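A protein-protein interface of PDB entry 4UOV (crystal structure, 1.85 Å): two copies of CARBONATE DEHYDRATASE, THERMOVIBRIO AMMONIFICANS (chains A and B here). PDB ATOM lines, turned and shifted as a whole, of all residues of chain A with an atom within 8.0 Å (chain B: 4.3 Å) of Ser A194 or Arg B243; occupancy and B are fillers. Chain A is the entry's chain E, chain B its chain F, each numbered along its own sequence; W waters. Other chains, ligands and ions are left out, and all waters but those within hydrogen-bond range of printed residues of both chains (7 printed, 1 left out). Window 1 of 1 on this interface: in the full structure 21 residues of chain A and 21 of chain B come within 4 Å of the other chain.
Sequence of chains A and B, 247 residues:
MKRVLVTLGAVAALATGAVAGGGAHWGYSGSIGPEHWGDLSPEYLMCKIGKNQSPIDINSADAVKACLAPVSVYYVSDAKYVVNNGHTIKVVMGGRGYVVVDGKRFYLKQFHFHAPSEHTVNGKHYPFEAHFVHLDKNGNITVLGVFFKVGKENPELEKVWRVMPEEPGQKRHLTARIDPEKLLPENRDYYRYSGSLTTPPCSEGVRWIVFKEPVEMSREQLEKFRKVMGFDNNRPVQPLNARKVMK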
ATOM      1  N   LYS A  51       5.251   2.137  18.673  1.00  0.00           N
ATOM      2  CA  LYS A  51       4.755   2.174  17.293  1.00  0.00           C
ATOM      3  C   LYS A  51       5.905   2.203  16.287  1.00  0.00           C
ATOM      4  O   LYS A  51       5.687   2.260  15.073  1.00  0.00           O
ATOM      5  CB  LYS A  51       3.841   3.390  17.074  1.00  0.00           C
ATOM      6  CG  LYS A  51       2.624   3.430  17.992  1.00  0.00           C
ATOM      7  CD  LYS A  51       1.663   2.287  17.718  1.00  0.00           C
ATOM      8  CE  LYS A  51       0.517   2.315  18.718  1.00  0.00           C
ATOM      9  NZ  LYS A  51      -0.190   1.004  18.766  1.00  0.00           N
ATOM     10  N   ASN A  52       7.133   2.138  16.800  1.00  0.00           N
ATOM     11  CA  ASN A  52       8.317   2.099  15.959  1.00  0.00           C
ATOM     12  C   ASN A  52       9.227   0.922  16.361  1.00  0.00           C
ATOM     13  O   ASN A  52      10.409   1.105  16.659  1.00  0.00           O
ATOM     14  CB  ASN A  52       9.042   3.446  16.055  1.00  0.00           C
ATOM     15  CG  ASN A  52       8.203   4.596  15.512  1.00  0.00           C
ATOM     16  OD1 ASN A  52       8.205   4.869  14.314  1.00  0.00           O
ATOM     17  ND2 ASN A  52       7.477   5.269  16.393  1.00  0.00           N
ATOM     18  N   GLN A  53       8.657  -0.284  16.357  1.00  0.00           N
ATOM     19  CA  GLN A  53       9.359  -1.483  16.811  1.00  0.00           C
ATOM     20  C   GLN A  53      10.065  -2.243  15.687  1.00  0.00           C
ATOM     21  O   GLN A  53       9.705  -2.125  14.501  1.00  0.00           O
ATOM     22  CB  GLN A  53       8.373  -2.414  17.546  1.00  0.00           C
ATOM     23  CG  GLN A  53       7.828  -1.814  18.832  1.00  0.00           C
ATOM     24  CD  GLN A  53       8.834  -1.955  19.959  1.00  0.00           C
ATOM     25  OE1 GLN A  53       9.108  -3.072  20.421  1.00  0.00           O
ATOM     26  NE2 GLN A  53       9.408  -0.828  20.394  1.00  0.00           N
ATOM     27  N   SER A  54      11.060  -3.039  16.086  1.00  0.00           N
ATOM     28  CA  SER A  54      11.804  -3.912  15.179  1.00  0.00           C
ATOM     29  C   SER A  54      11.699  -5.371  15.640  1.00  0.00           C
ATOM     30  O   SER A  54      11.464  -5.618  16.824  1.00  0.00           O
ATOM     31  CB  SER A  54      13.277  -3.506  15.175  1.00  0.00           C
ATOM     32  OG  SER A  54      13.429  -2.200  14.626  1.00  0.00           O
ATOM     33  N   ILE A  56      11.048  -5.803  11.196  1.00  0.00           N
ATOM     34  CA  ILE A  56       9.909  -5.582  10.315  1.00  0.00           C
ATOM     35  C   ILE A  56      10.043  -6.442   9.069  1.00  0.00           C
ATOM     36  O   ILE A  56      11.140  -6.948   8.768  1.00  0.00           O
ATOM     37  CB  ILE A  56       9.828  -4.098   9.858  1.00  0.00           C
ATOM     38  CG1 ILE A  56      11.100  -3.726   9.073  1.00  0.00           C
ATOM     39  CG2 ILE A  56       9.586  -3.174  11.060  1.00  0.00           C
ATOM     40  CD1 ILE A  56      11.083  -2.331   8.452  1.00  0.00           C
ATOM     41  N   ASP A 102      25.052   9.309   9.347  1.00  0.00           N
ATOM     42  CA  ASP A 102      24.658  10.705   9.604  1.00  0.00           C
ATOM     43  C   ASP A 102      25.866  11.566  10.028  1.00  0.00           C
ATOM     44  O   ASP A 102      25.747  12.431  10.904  1.00  0.00           O
ATOM     45  CB  ASP A 102      23.548  10.762  10.666  1.00  0.00           C
ATOM     46  CG  ASP A 102      22.275  10.032  10.222  1.00  0.00           C
ATOM     47  OD1 ASP A 102      22.050   9.916   8.995  1.00  0.00           O
ATOM     48  OD2 ASP A 102      21.499   9.597  11.096  1.00  0.00           O
ATOM     49  N   ARG A 192      17.221   1.396   5.022  1.00  0.00           N
ATOM     50  CA  ARG A 192      17.308   2.093   6.311  1.00  0.00           C
ATOM     51  C   ARG A 192      15.930   2.412   6.868  1.00  0.00           C
ATOM     52  O   ARG A 192      15.044   2.825   6.122  1.00  0.00           O
ATOM     53  CB  ARG A 192      18.124   3.404   6.211  1.00  0.00           C
ATOM     54  CG  ARG A 192      18.218   4.122   7.564  1.00  0.00           C
ATOM     55  CD  ARG A 192      19.081   5.381   7.524  1.00  0.00           C
ATOM     56  NE  ARG A 192      18.895   6.152   8.752  1.00  0.00           N
ATOM     57  CZ  ARG A 192      19.672   7.161   9.130  1.00  0.00           C
ATOM     58  NH1 ARG A 192      20.701   7.529   8.371  1.00  0.00           N
ATOM     59  NH2 ARG A 192      19.412   7.805  10.267  1.00  0.00           N
ATOM     60  N   TYR A 193      15.754   2.228   8.175  1.00  0.00           N
ATOM     61  CA  TYR A 193      14.549   2.698   8.872  1.00  0.00           C
ATOM     62  C   TYR A 193      14.883   2.977  10.340  1.00  0.00           C
ATOM     63  O   TYR A 193      15.974   2.624  10.820  1.00  0.00           O
ATOM     64  CB  TYR A 193      13.379   1.697   8.718  1.00  0.00           C
ATOM     65  CG  TYR A 193      13.513   0.442   9.560  1.00  0.00           C
ATOM     66  CD1 TYR A 193      14.409  -0.585   9.207  1.00  0.00           C
ATOM     67  CD2 TYR A 193      12.743   0.277  10.704  1.00  0.00           C
ATOM     68  CE1 TYR A 193      14.538  -1.728   9.993  1.00  0.00           C
ATOM     69  CE2 TYR A 193      12.861  -0.864  11.502  1.00  0.00           C
ATOM     70  CZ  TYR A 193      13.759  -1.858  11.147  1.00  0.00           C
ATOM     71  OH  TYR A 193      13.859  -2.995  11.952  1.00  0.00           O
ATOM     72  N   SER A 194      13.955   3.629  11.032  1.00  0.00           N
ATOM     73  CA  SER A 194      14.056   3.937  12.457  1.00  0.00           C
ATOM     74  C   SER A 194      13.244   2.900  13.234  1.00  0.00           C
ATOM     75  O   SER A 194      12.047   2.702  12.949  1.00  0.00           O
ATOM     76  CB  SER A 194      13.519   5.364  12.716  1.00  0.00           C
ATOM     77  OG  SER A 194      13.095   5.582  14.063  1.00  0.00           O
ATOM     78  N   GLY A 195      13.863   2.263  14.218  1.00  0.00           N
ATOM     79  CA  GLY A 195      13.185   1.204  14.943  1.00  0.00           C
ATOM     80  C   GLY A 195      13.615   1.045  16.381  1.00  0.00           C
ATOM     81  O   GLY A 195      13.770   2.029  17.109  1.00  0.00           O
ATOM     82  N   SER A 196      13.781  -0.212  16.794  1.00  0.00           N
ATOM     83  CA  SER A 196      14.014  -0.539  18.200  1.00  0.00           C
ATOM     84  C   SER A 196      15.001  -1.690  18.339  1.00  0.00           C
ATOM     85  O   SER A 196      15.346  -2.335  17.350  1.00  0.00           O
ATOM     86  CB  SER A 196      12.695  -0.945  18.893  1.00  0.00           C
ATOM     87  OG  SER A 196      12.326  -2.295  18.575  1.00  0.00           O
ATOM     88  N   GLU A 204      13.302   2.186  21.722  1.00  0.00           N
ATOM     89  CA  GLU A 204      13.211   2.781  20.396  1.00  0.00           C
ATOM     90  C   GLU A 204      14.310   3.827  20.218  1.00  0.00           C
ATOM     91  O   GLU A 204      15.216   3.908  21.049  1.00  0.00           O
ATOM     92  CB  GLU A 204      11.790   3.326  20.152  1.00  0.00           C
ATOM     93  CG  GLU A 204      10.785   2.174  20.019  1.00  0.00           C
ATOM     94  CD  GLU A 204       9.376   2.595  19.620  1.00  0.00           C
ATOM     95  OE1 GLU A 204       9.112   3.810  19.509  1.00  0.00           O
ATOM     96  OE2 GLU A 204       8.526   1.691  19.419  1.00  0.00           O
ATOM     97  N   GLY A 205      14.243   4.595  19.133  1.00  0.00           N
ATOM     98  CA  GLY A 205      15.331   5.493  18.725  1.00  0.00           C
ATOM     99  C   GLY A 205      16.580   4.787  18.180  1.00  0.00           C
ATOM    100  O   GLY A 205      17.675   5.338  18.243  1.00  0.00           O
ATOM    101  N   VAL A 206      16.416   3.588  17.623  1.00  0.00           N
ATOM    102  CA  VAL A 206      17.549   2.818  17.045  1.00  0.00           C
ATOM    103  C   VAL A 206      17.591   2.985  15.529  1.00  0.00           C
ATOM    104  O   VAL A 206      16.556   2.836  14.867  1.00  0.00           O
ATOM    105  CB  VAL A 206      17.406   1.302  17.386  1.00  0.00           C
ATOM    106  CG1 VAL A 206      18.552   0.482  16.769  1.00  0.00           C
ATOM    107  CG2 VAL A 206      17.359   1.118  18.904  1.00  0.00           C
ATOM    108  N   ARG A 207      18.770   3.307  14.988  1.00  0.00           N
ATOM    109  CA  ARG A 207      18.999   3.345  13.545  1.00  0.00           C
ATOM    110  C   ARG A 207      19.267   1.923  13.025  1.00  0.00           C
ATOM    111  O   ARG A 207      20.167   1.247  13.526  1.00  0.00           O
ATOM    112  CB  ARG A 207      20.211   4.237  13.221  1.00  0.00           C
ATOM    113  CG  ARG A 207      20.008   5.729  13.525  1.00  0.00           C
ATOM    114  CD  ARG A 207      21.381   6.399  13.619  1.00  0.00           C
ATOM    115  NE  ARG A 207      21.376   7.858  13.432  1.00  0.00           N
ATOM    116  CZ  ARG A 207      21.175   8.759  14.397  1.00  0.00           C
ATOM    117  NH1 ARG A 207      20.884   8.382  15.640  1.00  0.00           N
ATOM    118  NH2 ARG A 207      21.243  10.061  14.101  1.00  0.00           N
ATOM    119  N   TRP A 208      18.487   1.484  12.037  1.00  0.00           N
ATOM    120  CA  TRP A 208      18.694   0.196  11.377  1.00  0.00           C
ATOM    121  C   TRP A 208      19.229   0.361   9.963  1.00  0.00           C
ATOM    122  O   TRP A 208      18.635   1.074   9.131  1.00  0.00           O
ATOM    123  CB  TRP A 208      17.398  -0.631  11.359  1.00  0.00           C
ATOM    124  CG  TRP A 208      17.179  -1.355  12.668  1.00  0.00           C
ATOM    125  CD1 TRP A 208      16.426  -0.941  13.743  1.00  0.00           C
ATOM    126  CD2 TRP A 208      17.753  -2.616  13.035  1.00  0.00           C
ATOM    127  NE1 TRP A 208      16.506  -1.887  14.764  1.00  0.00           N
ATOM    128  CE2 TRP A 208      17.304  -2.922  14.344  1.00  0.00           C
ATOM    129  CE3 TRP A 208      18.594  -3.527  12.373  1.00  0.00           C
ATOM    130  CZ2 TRP A 208      17.685  -4.097  15.013  1.00  0.00           C
ATOM    131  CZ3 TRP A 208      18.970  -4.716  13.048  1.00  0.00           C
ATOM    132  CH2 TRP A 208      18.508  -4.978  14.347  1.00  0.00           C
ATOM    133  N   ILE A 209      20.358  -0.305   9.701  1.00  0.00           N
ATOM    134  CA  ILE A 209      20.969  -0.389   8.376  1.00  0.00           C
ATOM    135  C   ILE A 209      20.989  -1.875   8.007  1.00  0.00           C
ATOM    136  O   ILE A 209      21.786  -2.629   8.580  1.00  0.00           O
ATOM    137  CB  ILE A 209      22.428   0.135   8.393  1.00  0.00           C
ATOM    138  CG1 ILE A 209      22.509   1.588   8.932  1.00  0.00           C
ATOM    139  CG2 ILE A 209      23.076   0.009   7.010  1.00  0.00           C
ATOM    140  CD1 ILE A 209      21.855   2.638   8.043  1.00  0.00           C
ATOM    141  N   PRO A 239       4.539  -4.159  13.079  1.00  0.00           N
ATOM    142  CA  PRO A 239       3.921  -3.304  12.051  1.00  0.00           C
ATOM    143  C   PRO A 239       4.740  -2.043  11.761  1.00  0.00           C
ATOM    144  O   PRO A 239       5.263  -1.423  12.685  1.00  0.00           O
ATOM    145  CB  PRO A 239       2.590  -2.883  12.678  1.00  0.00           C
ATOM    146  CG  PRO A 239       2.360  -3.794  13.823  1.00  0.00           C
ATOM    147  CD  PRO A 239       3.683  -4.333  14.265  1.00  0.00           C
ATOM    148  N   LEU A 240       4.809  -1.659  10.489  1.00  0.00           N
ATOM    149  CA  LEU A 240       5.545  -0.455  10.086  1.00  0.00           C
ATOM    150  C   LEU A 240       4.896   0.800  10.644  1.00  0.00           C
ATOM    151  O   LEU A 240       5.587   1.772  10.979  1.00  0.00           O
ATOM    152  CB  LEU A 240       5.633  -0.342   8.557  1.00  0.00           C
ATOM    153  CG  LEU A 240       6.937  -0.760   7.891  1.00  0.00           C
ATOM    154  CD1 LEU A 240       6.859  -0.532   6.389  1.00  0.00           C
ATOM    155  CD2 LEU A 240       8.098   0.017   8.497  1.00  0.00           C
ATOM    156  N   ARG A 243       5.942   4.589   9.550  1.00  0.00           N
ATOM    157  CA  ARG A 243       7.286   4.633   8.951  1.00  0.00           C
ATOM    158  C   ARG A 243       7.362   4.257   7.475  1.00  0.00           C
ATOM    159  O   ARG A 243       6.552   3.475   6.970  1.00  0.00           O
ATOM    160  CB  ARG A 243       8.201   3.671   9.703  1.00  0.00           C
ATOM    161  CG  ARG A 243       8.360   3.997  11.172  1.00  0.00           C
ATOM    162  CD  ARG A 243       9.155   2.889  11.858  1.00  0.00           C
ATOM    163  NE  ARG A 243       8.342   1.700  12.118  1.00  0.00           N
ATOM    164  CZ  ARG A 243       8.785   0.619  12.757  1.00  0.00           C
ATOM    165  NH1 ARG A 243      10.035   0.577  13.248  1.00  0.00           N
ATOM    166  NH2 ARG A 243       7.968  -0.408  12.941  1.00  0.00           N
ATOM    167  N   LYS A 244       8.373   4.787   6.793  1.00  0.00           N
ATOM    168  CA  LYS A 244       8.760   4.243   5.501  1.00  0.00           C
ATOM    169  C   LYS A 244      10.176   3.722   5.614  1.00  0.00           C
ATOM    170  O   LYS A 244      10.983   4.258   6.381  1.00  0.00           O
ATOM    171  CB  LYS A 244       8.729   5.310   4.403  1.00  0.00           C
ATOM    172  CG  LYS A 244       7.340   5.833   4.079  1.00  0.00           C
ATOM    173  CD  LYS A 244       6.434   4.727   3.547  1.00  0.00           C
ATOM    174  CE  LYS A 244       6.354   4.733   2.031  1.00  0.00           C
ATOM    175  NZ  LYS A 244       5.301   3.770   1.592  1.00  0.00           N
ATOM    176  N   VAL A 245      10.470   2.694   4.831  1.00  0.00           N
ATOM    177  CA  VAL A 245      11.822   2.180   4.697  1.00  0.00           C
ATOM    178  C   VAL A 245      12.409   2.863   3.475  1.00  0.00           C
ATOM    179  O   VAL A 245      11.746   2.935   2.428  1.00  0.00           O
ATOM    180  CB  VAL A 245      11.801   0.653   4.453  1.00  0.00           C
ATOM    181  CG1 VAL A 245      13.223   0.110   4.298  1.00  0.00           C
ATOM    182  CG2 VAL A 245      11.078  -0.053   5.597  1.00  0.00           C
ATOM    183  N   MET A 246      13.641   3.362   3.601  1.00  0.00           N
ATOM    184  CA  MET A 246      14.352   3.910   2.443  1.00  0.00           C
ATOM    185  C   MET A 246      15.260   2.853   1.831  1.00  0.00           C
ATOM    186  O   MET A 246      15.822   2.017   2.543  1.00  0.00           O
ATOM    187  CB  MET A 246      15.151   5.161   2.815  1.00  0.00           C
ATOM    188  CG  MET A 246      14.278   6.393   3.042  1.00  0.00           C
ATOM    189  SD  MET A 246      15.327   7.819   3.405  1.00  0.00           S
ATOM    190  CE  MET A 246      15.906   7.435   5.060  1.00  0.00           C
ATOM    191  N   LYS B  51      10.647   8.554  21.529  1.00  0.00           N
ATOM    192  CA  LYS B  51      11.814   8.907  20.713  1.00  0.00           C
ATOM    193  C   LYS B  51      11.411   9.315  19.297  1.00  0.00           C
ATOM    194  O   LYS B  51      12.268   9.573  18.446  1.00  0.00           O
ATOM    195  CB  LYS B  51      12.809   7.732  20.633  1.00  0.00           C
ATOM    196  CG  LYS B  51      13.279   7.207  21.981  1.00  0.00           C
ATOM    197  CD  LYS B  51      14.025   8.280  22.753  1.00  0.00           C
ATOM    198  CE  LYS B  51      14.452   7.758  24.116  1.00  0.00           C
ATOM    199  NZ  LYS B  51      14.907   8.861  25.007  1.00  0.00           N
ATOM    200  N   ASN B  52      10.103   9.346  19.036  1.00  0.00           N
ATOM    201  CA  ASN B  52       9.602   9.720  17.718  1.00  0.00           C
ATOM    202  C   ASN B  52       8.520  10.811  17.844  1.00  0.00           C
ATOM    203  O   ASN B  52       7.406  10.659  17.340  1.00  0.00           O
ATOM    204  CB  ASN B  52       9.075   8.472  16.987  1.00  0.00           C
ATOM    205  CG  ASN B  52      10.181   7.469  16.679  1.00  0.00           C
ATOM    206  OD1 ASN B  52      10.833   7.572  15.653  1.00  0.00           O
ATOM    207  ND2 ASN B  52      10.401   6.511  17.574  1.00  0.00           N
ATOM    208  N   GLN B  53       8.874  11.901  18.522  1.00  0.00           N
ATOM    209  CA  GLN B  53       7.928  12.974  18.857  1.00  0.00           C
ATOM    210  C   GLN B  53       7.906  14.119  17.846  1.00  0.00           C
ATOM    211  O   GLN B  53       8.861  14.313  17.091  1.00  0.00           O
ATOM    212  CB  GLN B  53       8.237  13.506  20.260  1.00  0.00           C
ATOM    213  CG  GLN B  53       7.992  12.483  21.362  1.00  0.00           C
ATOM    214  CD  GLN B  53       6.519  12.383  21.700  1.00  0.00           C
ATOM    215  OE1 GLN B  53       5.932  13.326  22.250  1.00  0.00           O
ATOM    216  NE2 GLN B  53       5.903  11.243  21.362  1.00  0.00           N
ATOM    217  N   ILE B  56       9.203  18.975  14.911  1.00  0.00           N
ATOM    218  CA  ILE B  56      10.660  18.903  14.788  1.00  0.00           C
ATOM    219  C   ILE B  56      11.141  20.119  14.017  1.00  0.00           C
ATOM    220  O   ILE B  56      10.351  20.785  13.331  1.00  0.00           O
ATOM    221  CB  ILE B  56      11.109  17.628  14.039  1.00  0.00           C
ATOM    222  CG1 ILE B  56      10.491  17.572  12.639  1.00  0.00           C
ATOM    223  CG2 ILE B  56      10.774  16.375  14.854  1.00  0.00           C
ATOM    224  CD1 ILE B  56      11.211  16.600  11.712  1.00  0.00           C
ATOM    225  N   TYR B 193       7.864  12.692   7.473  1.00  0.00           N
ATOM    226  CA  TYR B 193       8.525  11.934   8.540  1.00  0.00           C
ATOM    227  C   TYR B 193       7.472  11.262   9.431  1.00  0.00           C
ATOM    228  O   TYR B 193       6.267  11.552   9.325  1.00  0.00           O
ATOM    229  CB  TYR B 193       9.483  12.833   9.369  1.00  0.00           C
ATOM    230  CG  TYR B 193       8.770  13.776  10.340  1.00  0.00           C
ATOM    231  CD1 TYR B 193       8.136  14.953   9.892  1.00  0.00           C
ATOM    232  CD2 TYR B 193       8.725  13.476  11.705  1.00  0.00           C
ATOM    233  CE1 TYR B 193       7.479  15.809  10.790  1.00  0.00           C
ATOM    234  CE2 TYR B 193       8.082  14.318  12.606  1.00  0.00           C
ATOM    235  CZ  TYR B 193       7.462  15.484  12.141  1.00  0.00           C
ATOM    236  OH  TYR B 193       6.827  16.282  13.063  1.00  0.00           O
ATOM    237  N   SER B 194       7.925  10.345  10.274  1.00  0.00           N
ATOM    238  CA  SER B 194       7.056   9.618  11.218  1.00  0.00           C
ATOM    239  C   SER B 194       7.196  10.266  12.603  1.00  0.00           C
ATOM    240  O   SER B 194       8.308  10.398  13.114  1.00  0.00           O
ATOM    241  CB  SER B 194       7.441   8.122  11.220  1.00  0.00           C
ATOM    242  OG  SER B 194       7.116   7.451  12.429  1.00  0.00           O
ATOM    243  N   GLY B 195       6.076  10.675  13.196  1.00  0.00           N
ATOM    244  CA  GLY B 195       6.101  11.406  14.460  1.00  0.00           C
ATOM    245  C   GLY B 195       4.906  11.142  15.368  1.00  0.00           C
ATOM    246  O   GLY B 195       4.464   9.997  15.528  1.00  0.00           O
ATOM    247  N   PRO B 239      13.704  16.223  19.502  1.00  0.00           N
ATOM    248  CA  PRO B 239      14.863  15.677  18.772  1.00  0.00           C
ATOM    249  C   PRO B 239      14.476  14.634  17.712  1.00  0.00           C
ATOM    250  O   PRO B 239      13.585  13.822  17.957  1.00  0.00           O
ATOM    251  CB  PRO B 239      15.713  15.024  19.873  1.00  0.00           C
ATOM    252  CG  PRO B 239      14.850  14.955  21.088  1.00  0.00           C
ATOM    253  CD  PRO B 239      13.784  16.010  20.961  1.00  0.00           C
ATOM    254  N   LEU B 240      15.143  14.675  16.555  1.00  0.00           N
ATOM    255  CA  LEU B 240      14.930  13.687  15.499  1.00  0.00           C
ATOM    256  C   LEU B 240      15.286  12.269  15.940  1.00  0.00           C
ATOM    257  O   LEU B 240      14.615  11.301  15.542  1.00  0.00           O
ATOM    258  CB  LEU B 240      15.726  14.035  14.242  1.00  0.00           C
ATOM    259  CG  LEU B 240      15.067  14.778  13.083  1.00  0.00           C
ATOM    260  CD1 LEU B 240      16.110  14.957  11.987  1.00  0.00           C
ATOM    261  CD2 LEU B 240      13.856  14.029  12.543  1.00  0.00           C
ATOM    262  N   ASN B 241      16.329  12.137  16.768  1.00  0.00           N
ATOM    263  CA  ASN B 241      16.821  10.816  17.225  1.00  0.00           C
ATOM    264  C   ASN B 241      17.240   9.945  16.018  1.00  0.00           C
ATOM    265  O   ASN B 241      18.071  10.380  15.221  1.00  0.00           O
ATOM    266  CB  ASN B 241      15.827  10.119  18.196  1.00  0.00           C
ATOM    267  CG  ASN B 241      15.637  10.907  19.488  1.00  0.00           C
ATOM    268  OD1 ASN B 241      16.617  11.381  20.070  1.00  0.00           O
ATOM    269  ND2 ASN B 241      14.381  11.071  19.937  1.00  0.00           N
ATOM    270  N   ALA B 242      16.648   8.762  15.847  1.00  0.00           N
ATOM    271  CA  ALA B 242      17.039   7.869  14.739  1.00  0.00           C
ATOM    272  C   ALA B 242      16.396   8.219  13.406  1.00  0.00           C
ATOM    273  O   ALA B 242      16.746   7.635  12.381  1.00  0.00           O
ATOM    274  CB  ALA B 242      16.738   6.403  15.080  1.00  0.00           C
ATOM    275  N   ARG B 243      15.438   9.145  13.408  1.00  0.00           N
ATOM    276  CA  ARG B 243      14.679   9.431  12.186  1.00  0.00           C
ATOM    277  C   ARG B 243      15.427  10.233  11.124  1.00  0.00           C
ATOM    278  O   ARG B 243      16.299  11.039  11.431  1.00  0.00           O
ATOM    279  CB  ARG B 243      13.400  10.189  12.548  1.00  0.00           C
ATOM    280  CG  ARG B 243      12.432   9.381  13.408  1.00  0.00           C
ATOM    281  CD  ARG B 243      11.279  10.274  13.871  1.00  0.00           C
ATOM    282  NE  ARG B 243      11.694  11.261  14.881  1.00  0.00           N
ATOM    283  CZ  ARG B 243      10.862  12.135  15.449  1.00  0.00           C
ATOM    284  NH1 ARG B 243       9.580  12.151  15.105  1.00  0.00           N
ATOM    285  NH2 ARG B 243      11.306  13.001  16.360  1.00  0.00           N
ATOM    286  N   LYS B 244      15.052  10.019   9.872  1.00  0.00           N
ATOM    287  CA  LYS B 244      15.373  10.949   8.792  1.00  0.00           C
ATOM    288  C   LYS B 244      14.082  11.561   8.250  1.00  0.00           C
ATOM    289  O   LYS B 244      13.023  10.907   8.225  1.00  0.00           O
ATOM    290  CB  LYS B 244      16.125  10.268   7.644  1.00  0.00           C
ATOM    291  CG  LYS B 244      17.508   9.718   8.019  1.00  0.00           C
ATOM    292  CD  LYS B 244      18.461  10.791   8.538  1.00  0.00           C
ATOM    293  CE  LYS B 244      19.261  11.421   7.416  1.00  0.00           C
ATOM    294  NZ  LYS B 244      20.279  12.378   7.941  1.00  0.00           N
HETATM  295  O   HOH W   1      19.597  12.731  15.244  1.00  0.00           O
HETATM  296  O   HOH W   2      12.515   4.423  16.782  1.00  0.00           O
HETATM  297  O   HOH W   3      10.066   6.600  13.347  1.00  0.00           O
HETATM  298  O   HOH W   4       9.341   6.260  20.689  1.00  0.00           O
HETATM  299  O   HOH W   5      20.786  10.847  17.247  1.00  0.00           O
HETATM  300  O   HOH W   6      17.560   5.259  11.185  1.00  0.00           O
HETATM  301  O   HOH W   7       5.920   7.665  15.086  1.00  0.00           O
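ND2 of Asn A52 lies close to ND2 of Asn B52, at 3.4 Å.
OG of Ser B194 is in hydrogen-bond range of OD1 of Asn A52 (3.4 Å).
NZ of Lys B244 lies within salt-bridge range of OD1 of Asp A102 (3.2 Å).
The backbone carbonyl oxygen (O) of Ala B242 lies within hydrogen-bond range of the guanidinium group (NH2) of Arg A192 (3.4 Å).
OG of Ser A194 sits at hydrogen-bond distance from OD1 of Asn B52, 3.4 Å away.
The guanidinium group (NH2) of Arg A207 sits at hydrogen-bond distance from the backbone carbonyl oxygen (O) of Asn B241 (3.4 Å).
The backbone NH (N) of Asn A52 is in hydrogen-bond range of the side-chain carboxylate (OE2) of Glu A204 (3.0 Å).
OD1 of Asp A102 lies within salt-bridge range of NH1 of Arg A192 (2.8 Å).
The backbone carbonyl oxygen (O) of Ser A194 lies within hydrogen-bond range of the guanidinium group (NH1) of Arg A243, at 2.9 Å.
O of Gly A195 sits at hydrogen-bond distance from N of Gly A205.
The backbone carbonyl oxygen of Asn B52 sits close to the guanidinium group of Arg B243 (3.5 Å).
Among the printed residues, pairs that only touch across the chains: Arg A192 with Lys B244 (3.5 Å), Ser A194 with Ala B242 (3.9 Å), Ser A194 with Arg B243 (3.9 Å), Glu A204 with Lys B51 (3.9 Å), Glu A204 with Asn B52 (3.6 Å), Gly A205 with Lys B51 (3.8 Å), Gly A205 with Ala B242 (3.5 Å), Val A206 with Ala B242 (3.6 Å), Arg A207 with Ala B242 (3.7 Å), Arg A243 with Ser B194 (3.9 Å) and Met A246 with Lys B244 (3.8 Å).
Printed residues of chain B within 4 Å of Ser A194: Asn B52 (3.4 Å), Ala B242 (3.9 Å) and Arg B243 (3.9 Å).
Of the printed residues of chain A, Arg B243 touches Ser A194 (3.9 Å).
Of the printed residues of chain B, Met A246 touches Lys B244 (3.8 Å).
Of the printed residues of chain B, Arg A207 touches Asn B241 and Ala B242.
Val A245 touches none of the printed residues of chain B.
The nearest printed residue of chain B that does not touch Ser A194 is Lys B244 (5.7 Å).
The nearest printed residue of chain B that does not touch Asn A52 is Gly B195 (5.7 Å).
Hydrophobic or aromatic side chains of chain B that line the printed part of chain A: Ala B242.
Of the 23 printed residues of chain A, 10 touch a printed residue of chain B.
Hydrophobic or aromatic side chains of chain A within 4 Å of the printed part of chain B: Met A246.
Among the printed residues, 17 pairs touch across the chains.
Asn B52 touches its own counterpart, Asn A52.
Asn A52 touches Ser B194, and with the chains exchanged Ser A194 touches Asn B52.
Ser A194 touches Arg B243, and with the chains exchanged Arg A243 touches Ser B194.
Positions printed for both chains: 51, 52, 53, 56, 193, 194, 195, 239, 240, 243 and 244.
Water W3 lies within hydrogen-bond range of the side-chain amide oxygen (OD1) of Asn B52 (2.6 Å), the side-chain amide oxygen (OD1) of Asn A52 (2.7 Å), the side-chain hydroxyl (OG) of Ser B194 (3.2 Å) and the side-chain hydroxyl (OG) of Ser A194 (3.3 Å).
Water W6 lies within hydrogen-bond range of the backbone carbonyl oxygen of Ala B242 (2.8 Å), the guanidinium group of Arg A192 (2.9 Å) and the backbone carbonyl oxygen of Tyr A193 (3.1 Å).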
